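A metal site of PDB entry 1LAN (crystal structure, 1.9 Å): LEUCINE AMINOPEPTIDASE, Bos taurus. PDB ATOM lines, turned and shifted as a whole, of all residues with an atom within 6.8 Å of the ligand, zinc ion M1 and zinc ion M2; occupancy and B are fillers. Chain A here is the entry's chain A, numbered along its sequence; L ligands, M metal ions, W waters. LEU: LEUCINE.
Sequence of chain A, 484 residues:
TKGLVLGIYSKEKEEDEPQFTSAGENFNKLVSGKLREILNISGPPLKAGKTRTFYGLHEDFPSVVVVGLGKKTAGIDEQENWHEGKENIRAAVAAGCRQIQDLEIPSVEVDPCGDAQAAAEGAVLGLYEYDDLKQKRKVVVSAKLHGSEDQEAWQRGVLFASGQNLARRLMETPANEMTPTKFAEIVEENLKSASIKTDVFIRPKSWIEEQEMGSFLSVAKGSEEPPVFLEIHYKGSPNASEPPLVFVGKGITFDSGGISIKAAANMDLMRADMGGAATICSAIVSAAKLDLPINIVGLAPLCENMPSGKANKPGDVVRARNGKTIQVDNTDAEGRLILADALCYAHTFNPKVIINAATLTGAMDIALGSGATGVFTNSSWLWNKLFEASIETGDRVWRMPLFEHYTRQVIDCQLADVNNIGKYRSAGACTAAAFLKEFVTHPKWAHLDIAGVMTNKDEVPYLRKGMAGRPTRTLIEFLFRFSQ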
ATOM      1  N   LYS A 250     -11.015  20.149   8.180  1.00  0.00           N
ATOM      2  CA  LYS A 250     -12.183  19.354   7.761  1.00  0.00           C
ATOM      3  C   LYS A 250     -11.962  18.900   6.295  1.00  0.00           C
ATOM      4  O   LYS A 250     -11.833  19.746   5.393  1.00  0.00           O
ATOM      5  CB  LYS A 250     -13.464  20.199   7.851  1.00  0.00           C
ATOM      6  CG  LYS A 250     -14.690  19.569   7.211  1.00  0.00           C
ATOM      7  CD  LYS A 250     -15.836  20.579   7.095  1.00  0.00           C
ATOM      8  CE  LYS A 250     -17.047  19.959   6.384  1.00  0.00           C
ATOM      9  NZ  LYS A 250     -18.179  20.931   6.262  1.00  0.00           N
ATOM     10  N   ILE A 252     -13.998  16.950   3.930  1.00  0.00           N
ATOM     11  CA  ILE A 252     -15.115  16.280   3.286  1.00  0.00           C
ATOM     12  C   ILE A 252     -14.876  16.506   1.783  1.00  0.00           C
ATOM     13  O   ILE A 252     -15.016  17.619   1.294  1.00  0.00           O
ATOM     14  CB  ILE A 252     -16.468  16.880   3.739  1.00  0.00           C
ATOM     15  CG1 ILE A 252     -16.697  16.579   5.234  1.00  0.00           C
ATOM     16  CG2 ILE A 252     -17.642  16.330   2.871  1.00  0.00           C
ATOM     17  CD1 ILE A 252     -16.987  15.109   5.540  1.00  0.00           C
ATOM     18  N   ASP A 255     -19.736  16.811  -0.206  1.00  0.00           N
ATOM     19  CA  ASP A 255     -20.869  16.874   0.722  1.00  0.00           C
ATOM     20  C   ASP A 255     -22.215  16.992  -0.012  1.00  0.00           C
ATOM     21  O   ASP A 255     -22.569  18.056  -0.542  1.00  0.00           O
ATOM     22  CB  ASP A 255     -20.690  18.057   1.687  1.00  0.00           C
ATOM     23  CG  ASP A 255     -21.719  18.042   2.828  1.00  0.00           C
ATOM     24  OD1 ASP A 255     -22.341  16.991   3.087  1.00  0.00           O
ATOM     25  OD2 ASP A 255     -21.880  19.101   3.469  1.00  0.00           O
ATOM     26  N   SER A 256     -22.957  15.880  -0.040  1.00  0.00           N
ATOM     27  CA  SER A 256     -24.279  15.824  -0.654  1.00  0.00           C
ATOM     28  C   SER A 256     -25.303  16.152   0.434  1.00  0.00           C
ATOM     29  O   SER A 256     -26.479  16.442   0.149  1.00  0.00           O
ATOM     30  CB  SER A 256     -24.558  14.413  -1.171  1.00  0.00           C
ATOM     31  OG  SER A 256     -24.811  13.502  -0.107  1.00  0.00           O
ATOM     32  N   GLY A 257     -24.872  16.081   1.691  1.00  0.00           N
ATOM     33  CA  GLY A 257     -25.752  16.322   2.823  1.00  0.00           C
ATOM     34  C   GLY A 257     -26.175  15.015   3.495  1.00  0.00           C
ATOM     35  O   GLY A 257     -26.545  15.016   4.690  1.00  0.00           O
ATOM     36  N   LYS A 262     -28.976  17.808   0.365  1.00  0.00           N
ATOM     37  CA  LYS A 262     -28.929  19.188  -0.100  1.00  0.00           C
ATOM     38  C   LYS A 262     -29.760  19.389  -1.365  1.00  0.00           C
ATOM     39  O   LYS A 262     -30.062  18.434  -2.076  1.00  0.00           O
ATOM     40  CB  LYS A 262     -27.479  19.598  -0.425  1.00  0.00           C
ATOM     41  CG  LYS A 262     -26.526  19.705   0.764  1.00  0.00           C
ATOM     42  CD  LYS A 262     -25.118  20.067   0.265  1.00  0.00           C
ATOM     43  CE  LYS A 262     -24.132  20.219   1.425  1.00  0.00           C
ATOM     44  NZ  LYS A 262     -24.549  21.307   2.354  1.00  0.00           N
ATOM     45  N   MET A 270     -19.735  21.873  -3.585  1.00  0.00           N
ATOM     46  CA  MET A 270     -19.424  21.049  -2.413  1.00  0.00           C
ATOM     47  C   MET A 270     -18.209  20.141  -2.589  1.00  0.00           C
ATOM     48  O   MET A 270     -17.792  19.453  -1.634  1.00  0.00           O
ATOM     49  CB  MET A 270     -20.654  20.257  -1.912  1.00  0.00           C
ATOM     50  CG  MET A 270     -21.768  21.143  -1.310  1.00  0.00           C
ATOM     51  SD  MET A 270     -21.235  22.224   0.041  1.00  0.00           S
ATOM     52  CE  MET A 270     -21.047  23.787  -0.772  1.00  0.00           C
ATOM     53  N   ASP A 273     -15.628  21.169  -0.101  1.00  0.00           N
ATOM     54  CA  ASP A 273     -15.917  21.043   1.327  1.00  0.00           C
ATOM     55  C   ASP A 273     -14.732  20.427   2.105  1.00  0.00           C
ATOM     56  O   ASP A 273     -14.856  20.028   3.276  1.00  0.00           O
ATOM     57  CB  ASP A 273     -17.211  20.248   1.528  1.00  0.00           C
ATOM     58  CG  ASP A 273     -17.920  20.581   2.843  1.00  0.00           C
ATOM     59  OD1 ASP A 273     -17.841  21.741   3.322  1.00  0.00           O
ATOM     60  OD2 ASP A 273     -18.568  19.665   3.397  1.00  0.00           O
ATOM     61  N   ASN A 305     -19.697  12.506   2.223  1.00  0.00           N
ATOM     62  CA  ASN A 305     -20.955  12.469   2.966  1.00  0.00           C
ATOM     63  C   ASN A 305     -22.026  12.171   1.903  1.00  0.00           C
ATOM     64  O   ASN A 305     -22.447  13.078   1.176  1.00  0.00           O
ATOM     65  CB  ASN A 305     -21.205  13.814   3.641  1.00  0.00           C
ATOM     66  CG  ASN A 305     -22.408  13.798   4.602  1.00  0.00           C
ATOM     67  OD1 ASN A 305     -23.036  14.843   4.847  1.00  0.00           O
ATOM     68  ND2 ASN A 305     -22.723  12.629   5.151  1.00  0.00           N
ATOM     69  N   ASN A 330     -29.166  16.359  12.225  1.00  0.00           N
ATOM     70  CA  ASN A 330     -29.093  16.717  10.809  1.00  0.00           C
ATOM     71  C   ASN A 330     -27.764  16.150  10.261  1.00  0.00           C
ATOM     72  O   ASN A 330     -26.686  16.538  10.719  1.00  0.00           O
ATOM     73  CB  ASN A 330     -29.147  18.245  10.617  1.00  0.00           C
ATOM     74  CG  ASN A 330     -29.266  18.649   9.143  1.00  0.00           C
ATOM     75  OD1 ASN A 330     -28.435  18.295   8.322  1.00  0.00           O
ATOM     76  ND2 ASN A 330     -30.349  19.335   8.807  1.00  0.00           N
ATOM     77  N   THR A 331     -27.849  15.224   9.307  1.00  0.00           N
ATOM     78  CA  THR A 331     -26.655  14.598   8.733  1.00  0.00           C
ATOM     79  C   THR A 331     -25.768  15.521   7.883  1.00  0.00           C
ATOM     80  O   THR A 331     -24.638  15.160   7.543  1.00  0.00           O
ATOM     81  CB  THR A 331     -27.020  13.311   7.934  1.00  0.00           C
ATOM     82  OG1 THR A 331     -27.676  13.667   6.712  1.00  0.00           O
ATOM     83  CG2 THR A 331     -27.984  12.435   8.737  1.00  0.00           C
ATOM     84  N   ASP A 332     -26.272  16.704   7.547  1.00  0.00           N
ATOM     85  CA  ASP A 332     -25.531  17.678   6.745  1.00  0.00           C
ATOM     86  C   ASP A 332     -24.663  18.568   7.658  1.00  0.00           C
ATOM     87  O   ASP A 332     -23.927  19.433   7.179  1.00  0.00           O
ATOM     88  CB  ASP A 332     -26.494  18.501   5.873  1.00  0.00           C
ATOM     89  CG  ASP A 332     -25.786  19.281   4.739  1.00  0.00           C
ATOM     90  OD1 ASP A 332     -24.597  19.049   4.435  1.00  0.00           O
ATOM     91  OD2 ASP A 332     -26.456  20.140   4.141  1.00  0.00           O
ATOM     92  N   ALA A 333     -24.774  18.388   8.972  1.00  0.00           N
ATOM     93  CA  ALA A 333     -23.914  19.133   9.906  1.00  0.00           C
ATOM     94  C   ALA A 333     -22.833  18.092  10.224  1.00  0.00           C
ATOM     95  O   ALA A 333     -22.587  17.733  11.393  1.00  0.00           O
ATOM     96  CB  ALA A 333     -24.704  19.509  11.183  1.00  0.00           C
ATOM     97  N   GLU A 334     -22.196  17.586   9.168  1.00  0.00           N
ATOM     98  CA  GLU A 334     -21.181  16.530   9.298  1.00  0.00           C
ATOM     99  C   GLU A 334     -19.761  16.975   9.641  1.00  0.00           C
ATOM    100  O   GLU A 334     -18.982  16.195  10.168  1.00  0.00           O
ATOM    101  CB  GLU A 334     -21.193  15.615   8.048  1.00  0.00           C
ATOM    102  CG  GLU A 334     -20.356  16.099   6.829  1.00  0.00           C
ATOM    103  CD  GLU A 334     -20.788  17.444   6.243  1.00  0.00           C
ATOM    104  OE1 GLU A 334     -22.014  17.737   6.189  1.00  0.00           O
ATOM    105  OE2 GLU A 334     -19.898  18.227   5.791  1.00  0.00           O
ATOM    106  N   GLY A 335     -19.418  18.220   9.339  1.00  0.00           N
ATOM    107  CA  GLY A 335     -18.076  18.689   9.616  1.00  0.00           C
ATOM    108  C   GLY A 335     -17.756  18.712  11.090  1.00  0.00           C
ATOM    109  O   GLY A 335     -16.652  18.319  11.492  1.00  0.00           O
ATOM    110  N   ARG A 336     -18.714  19.129  11.902  1.00  0.00           N
ATOM    111  CA  ARG A 336     -18.475  19.186  13.347  1.00  0.00           C
ATOM    112  C   ARG A 336     -18.311  17.782  13.920  1.00  0.00           C
ATOM    113  O   ARG A 336     -17.597  17.592  14.910  1.00  0.00           O
ATOM    114  CB  ARG A 336     -19.535  20.010  14.084  1.00  0.00           C
ATOM    115  CG  ARG A 336     -20.917  19.409  14.221  1.00  0.00           C
ATOM    116  CD  ARG A 336     -21.891  20.498  14.654  1.00  0.00           C
ATOM    117  NE  ARG A 336     -22.260  21.345  13.529  1.00  0.00           N
ATOM    118  CZ  ARG A 336     -23.101  22.378  13.581  1.00  0.00           C
ATOM    119  NH1 ARG A 336     -23.623  22.744  14.733  1.00  0.00           N
ATOM    120  NH2 ARG A 336     -23.385  23.055  12.481  1.00  0.00           N
ATOM    121  N   ALA A 358     -12.227  25.115   8.663  1.00  0.00           N
ATOM    122  CA  ALA A 358     -13.309  24.339   8.061  1.00  0.00           C
ATOM    123  C   ALA A 358     -14.309  25.185   7.283  1.00  0.00           C
ATOM    124  O   ALA A 358     -14.593  26.322   7.679  1.00  0.00           O
ATOM    125  CB  ALA A 358     -14.037  23.547   9.158  1.00  0.00           C
ATOM    126  N   THR A 359     -14.762  24.667   6.146  1.00  0.00           N
ATOM    127  CA  THR A 359     -15.799  25.314   5.322  1.00  0.00           C
ATOM    128  C   THR A 359     -17.034  24.753   6.042  1.00  0.00           C
ATOM    129  O   THR A 359     -17.729  23.873   5.542  1.00  0.00           O
ATOM    130  CB  THR A 359     -15.773  24.776   3.860  1.00  0.00           C
ATOM    131  OG1 THR A 359     -15.685  23.340   3.900  1.00  0.00           O
ATOM    132  CG2 THR A 359     -14.559  25.301   3.084  1.00  0.00           C
ATOM    133  N   LEU A 360     -17.277  25.266   7.250  1.00  0.00           N
ATOM    134  CA  LEU A 360     -18.304  24.715   8.112  1.00  0.00           C
ATOM    135  C   LEU A 360     -19.779  25.078   8.002  1.00  0.00           C
ATOM    136  O   LEU A 360     -20.605  24.185   7.943  1.00  0.00           O
ATOM    137  CB  LEU A 360     -17.841  24.849   9.575  1.00  0.00           C
ATOM    138  CG  LEU A 360     -18.408  23.909  10.648  1.00  0.00           C
ATOM    139  CD1 LEU A 360     -18.001  22.460  10.332  1.00  0.00           C
ATOM    140  CD2 LEU A 360     -17.883  24.305  12.026  1.00  0.00           C
ATOM    141  N   THR A 361     -20.112  26.363   7.980  1.00  0.00           N
ATOM    142  CA  THR A 361     -21.532  26.701   7.971  1.00  0.00           C
ATOM    143  C   THR A 361     -21.946  27.673   6.897  1.00  0.00           C
ATOM    144  O   THR A 361     -21.199  28.590   6.555  1.00  0.00           O
ATOM    145  CB  THR A 361     -21.942  27.322   9.327  1.00  0.00           C
ATOM    146  OG1 THR A 361     -21.255  28.563   9.518  1.00  0.00           O
ATOM    147  CG2 THR A 361     -21.606  26.396  10.492  1.00  0.00           C
ATOM    148  N   GLY A 362     -23.179  27.507   6.409  1.00  0.00           N
ATOM    149  CA  GLY A 362     -23.716  28.438   5.434  1.00  0.00           C
ATOM    150  C   GLY A 362     -23.934  29.766   6.177  1.00  0.00           C
ATOM    151  O   GLY A 362     -23.841  30.847   5.573  1.00  0.00           O
ATOM    152  N   ALA A 363     -24.163  29.677   7.483  1.00  0.00           N
ATOM    153  CA  ALA A 363     -24.385  30.862   8.319  1.00  0.00           C
ATOM    154  C   ALA A 363     -23.181  31.822   8.320  1.00  0.00           C
ATOM    155  O   ALA A 363     -23.360  33.038   8.411  1.00  0.00           O
ATOM    156  CB  ALA A 363     -24.739  30.461   9.768  1.00  0.00           C
ATOM    157  N   ASP A 365     -21.190  32.353   5.788  1.00  0.00           N
ATOM    158  CA  ASP A 365     -21.249  33.086   4.527  1.00  0.00           C
ATOM    159  C   ASP A 365     -22.297  34.202   4.630  1.00  0.00           C
ATOM    160  O   ASP A 365     -22.070  35.341   4.215  1.00  0.00           O
ATOM    161  CB  ASP A 365     -21.543  32.150   3.351  1.00  0.00           C
ATOM    162  CG  ASP A 365     -21.557  32.888   2.020  1.00  0.00           C
ATOM    163  OD1 ASP A 365     -20.550  33.519   1.672  1.00  0.00           O
ATOM    164  OD2 ASP A 365     -22.612  32.902   1.351  1.00  0.00           O
ATOM    165  N   ASP A 449     -13.721  29.457  10.412  1.00  0.00           N
ATOM    166  CA  ASP A 449     -14.827  29.030   9.535  1.00  0.00           C
ATOM    167  C   ASP A 449     -14.598  29.788   8.227  1.00  0.00           C
ATOM    168  O   ASP A 449     -14.811  30.994   8.158  1.00  0.00           O
ATOM    169  CB  ASP A 449     -16.199  29.359  10.138  1.00  0.00           C
ATOM    170  CG  ASP A 449     -17.353  28.656   9.418  1.00  0.00           C
ATOM    171  OD1 ASP A 449     -17.189  28.259   8.242  1.00  0.00           O
ATOM    172  OD2 ASP A 449     -18.436  28.493  10.036  1.00  0.00           O
ATOM    173  N   ILE A 450     -14.180  29.053   7.199  1.00  0.00           N
ATOM    174  CA  ILE A 450     -13.860  29.631   5.880  1.00  0.00           C
ATOM    175  C   ILE A 450     -14.893  29.403   4.777  1.00  0.00           C
ATOM    176  O   ILE A 450     -14.605  29.586   3.598  1.00  0.00           O
ATOM    177  CB  ILE A 450     -12.478  29.097   5.404  1.00  0.00           C
ATOM    178  CG1 ILE A 450     -12.541  27.593   5.151  1.00  0.00           C
ATOM    179  CG2 ILE A 450     -11.406  29.384   6.476  1.00  0.00           C
ATOM    180  CD1 ILE A 450     -11.383  27.064   4.345  1.00  0.00           C
ATOM    181  N   ALA A 451     -16.128  29.054   5.169  1.00  0.00           N
ATOM    182  CA  ALA A 451     -17.216  28.803   4.228  1.00  0.00           C
ATOM    183  C   ALA A 451     -17.498  30.020   3.318  1.00  0.00           C
ATOM    184  O   ALA A 451     -17.750  29.860   2.125  1.00  0.00           O
ATOM    185  CB  ALA A 451     -18.491  28.382   4.960  1.00  0.00           C
ATOM    186  N   GLY A 452     -17.399  31.215   3.875  1.00  0.00           N
ATOM    187  CA  GLY A 452     -17.634  32.424   3.102  1.00  0.00           C
ATOM    188  C   GLY A 452     -16.509  32.825   2.151  1.00  0.00           C
ATOM    189  O   GLY A 452     -16.748  33.564   1.207  1.00  0.00           O
ATOM    190  N   MET A 454     -14.689  30.584   0.472  1.00  0.00           N
ATOM    191  CA  MET A 454     -14.421  29.368  -0.304  1.00  0.00           C
ATOM    192  C   MET A 454     -14.187  29.684  -1.781  1.00  0.00           C
ATOM    193  O   MET A 454     -13.299  29.129  -2.427  1.00  0.00           O
ATOM    194  CB  MET A 454     -15.572  28.334  -0.139  1.00  0.00           C
ATOM    195  CG  MET A 454     -15.227  26.930  -0.623  1.00  0.00           C
ATOM    196  SD  MET A 454     -16.544  25.665  -0.485  1.00  0.00           S
ATOM    197  CE  MET A 454     -17.578  26.164  -1.816  1.00  0.00           C
HETATM  198  N   LEU L   1     -20.573  22.023   3.735  1.00  0.00           N
HETATM  199  CA  LEU L   1     -21.219  22.864   4.763  1.00  0.00           C
HETATM  200  C   LEU L   1     -22.101  21.944   5.663  1.00  0.00           C
HETATM  201  O   LEU L   1     -21.394  20.792   6.051  1.00  0.00           O
HETATM  202  CB  LEU L   1     -22.103  23.910   4.093  1.00  0.00           C
HETATM  203  CG  LEU L   1     -21.356  24.889   3.179  1.00  0.00           C
HETATM  204  CD1 LEU L   1     -22.151  26.093   2.775  1.00  0.00           C
HETATM  205  CD2 LEU L   1     -19.985  25.292   3.670  1.00  0.00           C
HETATM  206  OXT LEU L   1     -23.151  21.399   4.847  1.00  0.00           O
HETATM  207 ZN    ZN M   1     -19.789  20.128   4.950  1.00  0.00          ZN
HETATM  208 ZN    ZN M   2     -22.824  19.357   5.316  1.00  0.00          ZN
HETATM  209  O   HOH W   1     -25.622  22.724   6.846  1.00  0.00           O
HETATM  210  O   HOH W   2     -20.494  20.791   8.384  1.00  0.00           O
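Thr 359 touches the ligand.
Leu 360 touches the ligand.
Gly 362 touches the ligand (CA to CD1, 3.9 Å).
Ala 451 touches the ligand (CB to CD2, 3.7 Å).
Hydrophobic or aromatic side chains that line the ligand: Met 270 and Ala 451.
NZ of Lys 262 touches zinc ion M2 (3.9 Å).
The side-chain amino group of Lys 262 sits close to an oxygen (OXT) of the ligand (2.9 Å).
The side-chain sulfur (SD) of Met 270 lies close to a nitrogen (N) of the ligand.
Zinc ion M2 is bound by the side-chain carboxylate (OD1) of Asp 332 (2.0 Å), the side-chain carboxylate (OE1) of Glu 334 (2.0 Å), the side-chain carboxylate (OD2) of Asp 255 (2.1 Å), an oxygen (OXT) of the ligand (2.1 Å), an oxygen (O) of the ligand (2.2 Å) and the backbone carbonyl oxygen (O) of Asp 332 (2.2 Å).
Zinc ion M2 has six donor atoms within binding distance.
Zinc ion M1 is bound by OD2 of Asp 273 (2.0 Å), O of the ligand (2.1 Å), OE2 of Glu 334 (2.1 Å), NZ of Lys 250 (2.2 Å) and N of the ligand (2.4 Å).
Slightly farther from zinc ion M1 lies OD2 of Asp 255 (2.8 Å).
Four residues have an atom within 4 Å of zinc ion M1: Lys 250, Asp 255, Asp 273 and Glu 334.
Water W2 lies within hydrogen-bond range of the backbone NH (N) of Gly 335 and the backbone carbonyl oxygen (O) of Leu 360.
The side-chain carboxylate (OD2) of Asp 332 is in salt-bridge range of the side-chain amino group (NZ) of Lys 262 (2.9 Å).
The backbone NH of Asp 332 lies within hydrogen-bond range of the side-chain amide oxygen of Asn 330 (2.8 Å).
The side-chain carboxylate (OD1) of Asp 273 is in hydrogen-bond range of the side-chain hydroxyl (OG1) of Thr 359.
The side-chain amide oxygen (OD1) of Asn 305 lies close to the side-chain carboxylate (OD1) of Asp 255, 2.9 Å away.
The side-chain amino group of Lys 250 lies close to the backbone carbonyl oxygen of Thr 359, at 3.1 Å.
The backbone NH of Lys 262 sits at hydrogen-bond distance from the backbone carbonyl oxygen of Ser 256 (2.9 Å).
The backbone NH (N) of Leu 360 sits at hydrogen-bond distance from the side-chain carboxylate (OD1) of Asp 449, at 3.2 Å.
The side-chain carboxylate (OD1) of Asp 449 is in hydrogen-bond range of the backbone NH (N) of Ala 451 (3.3 Å).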
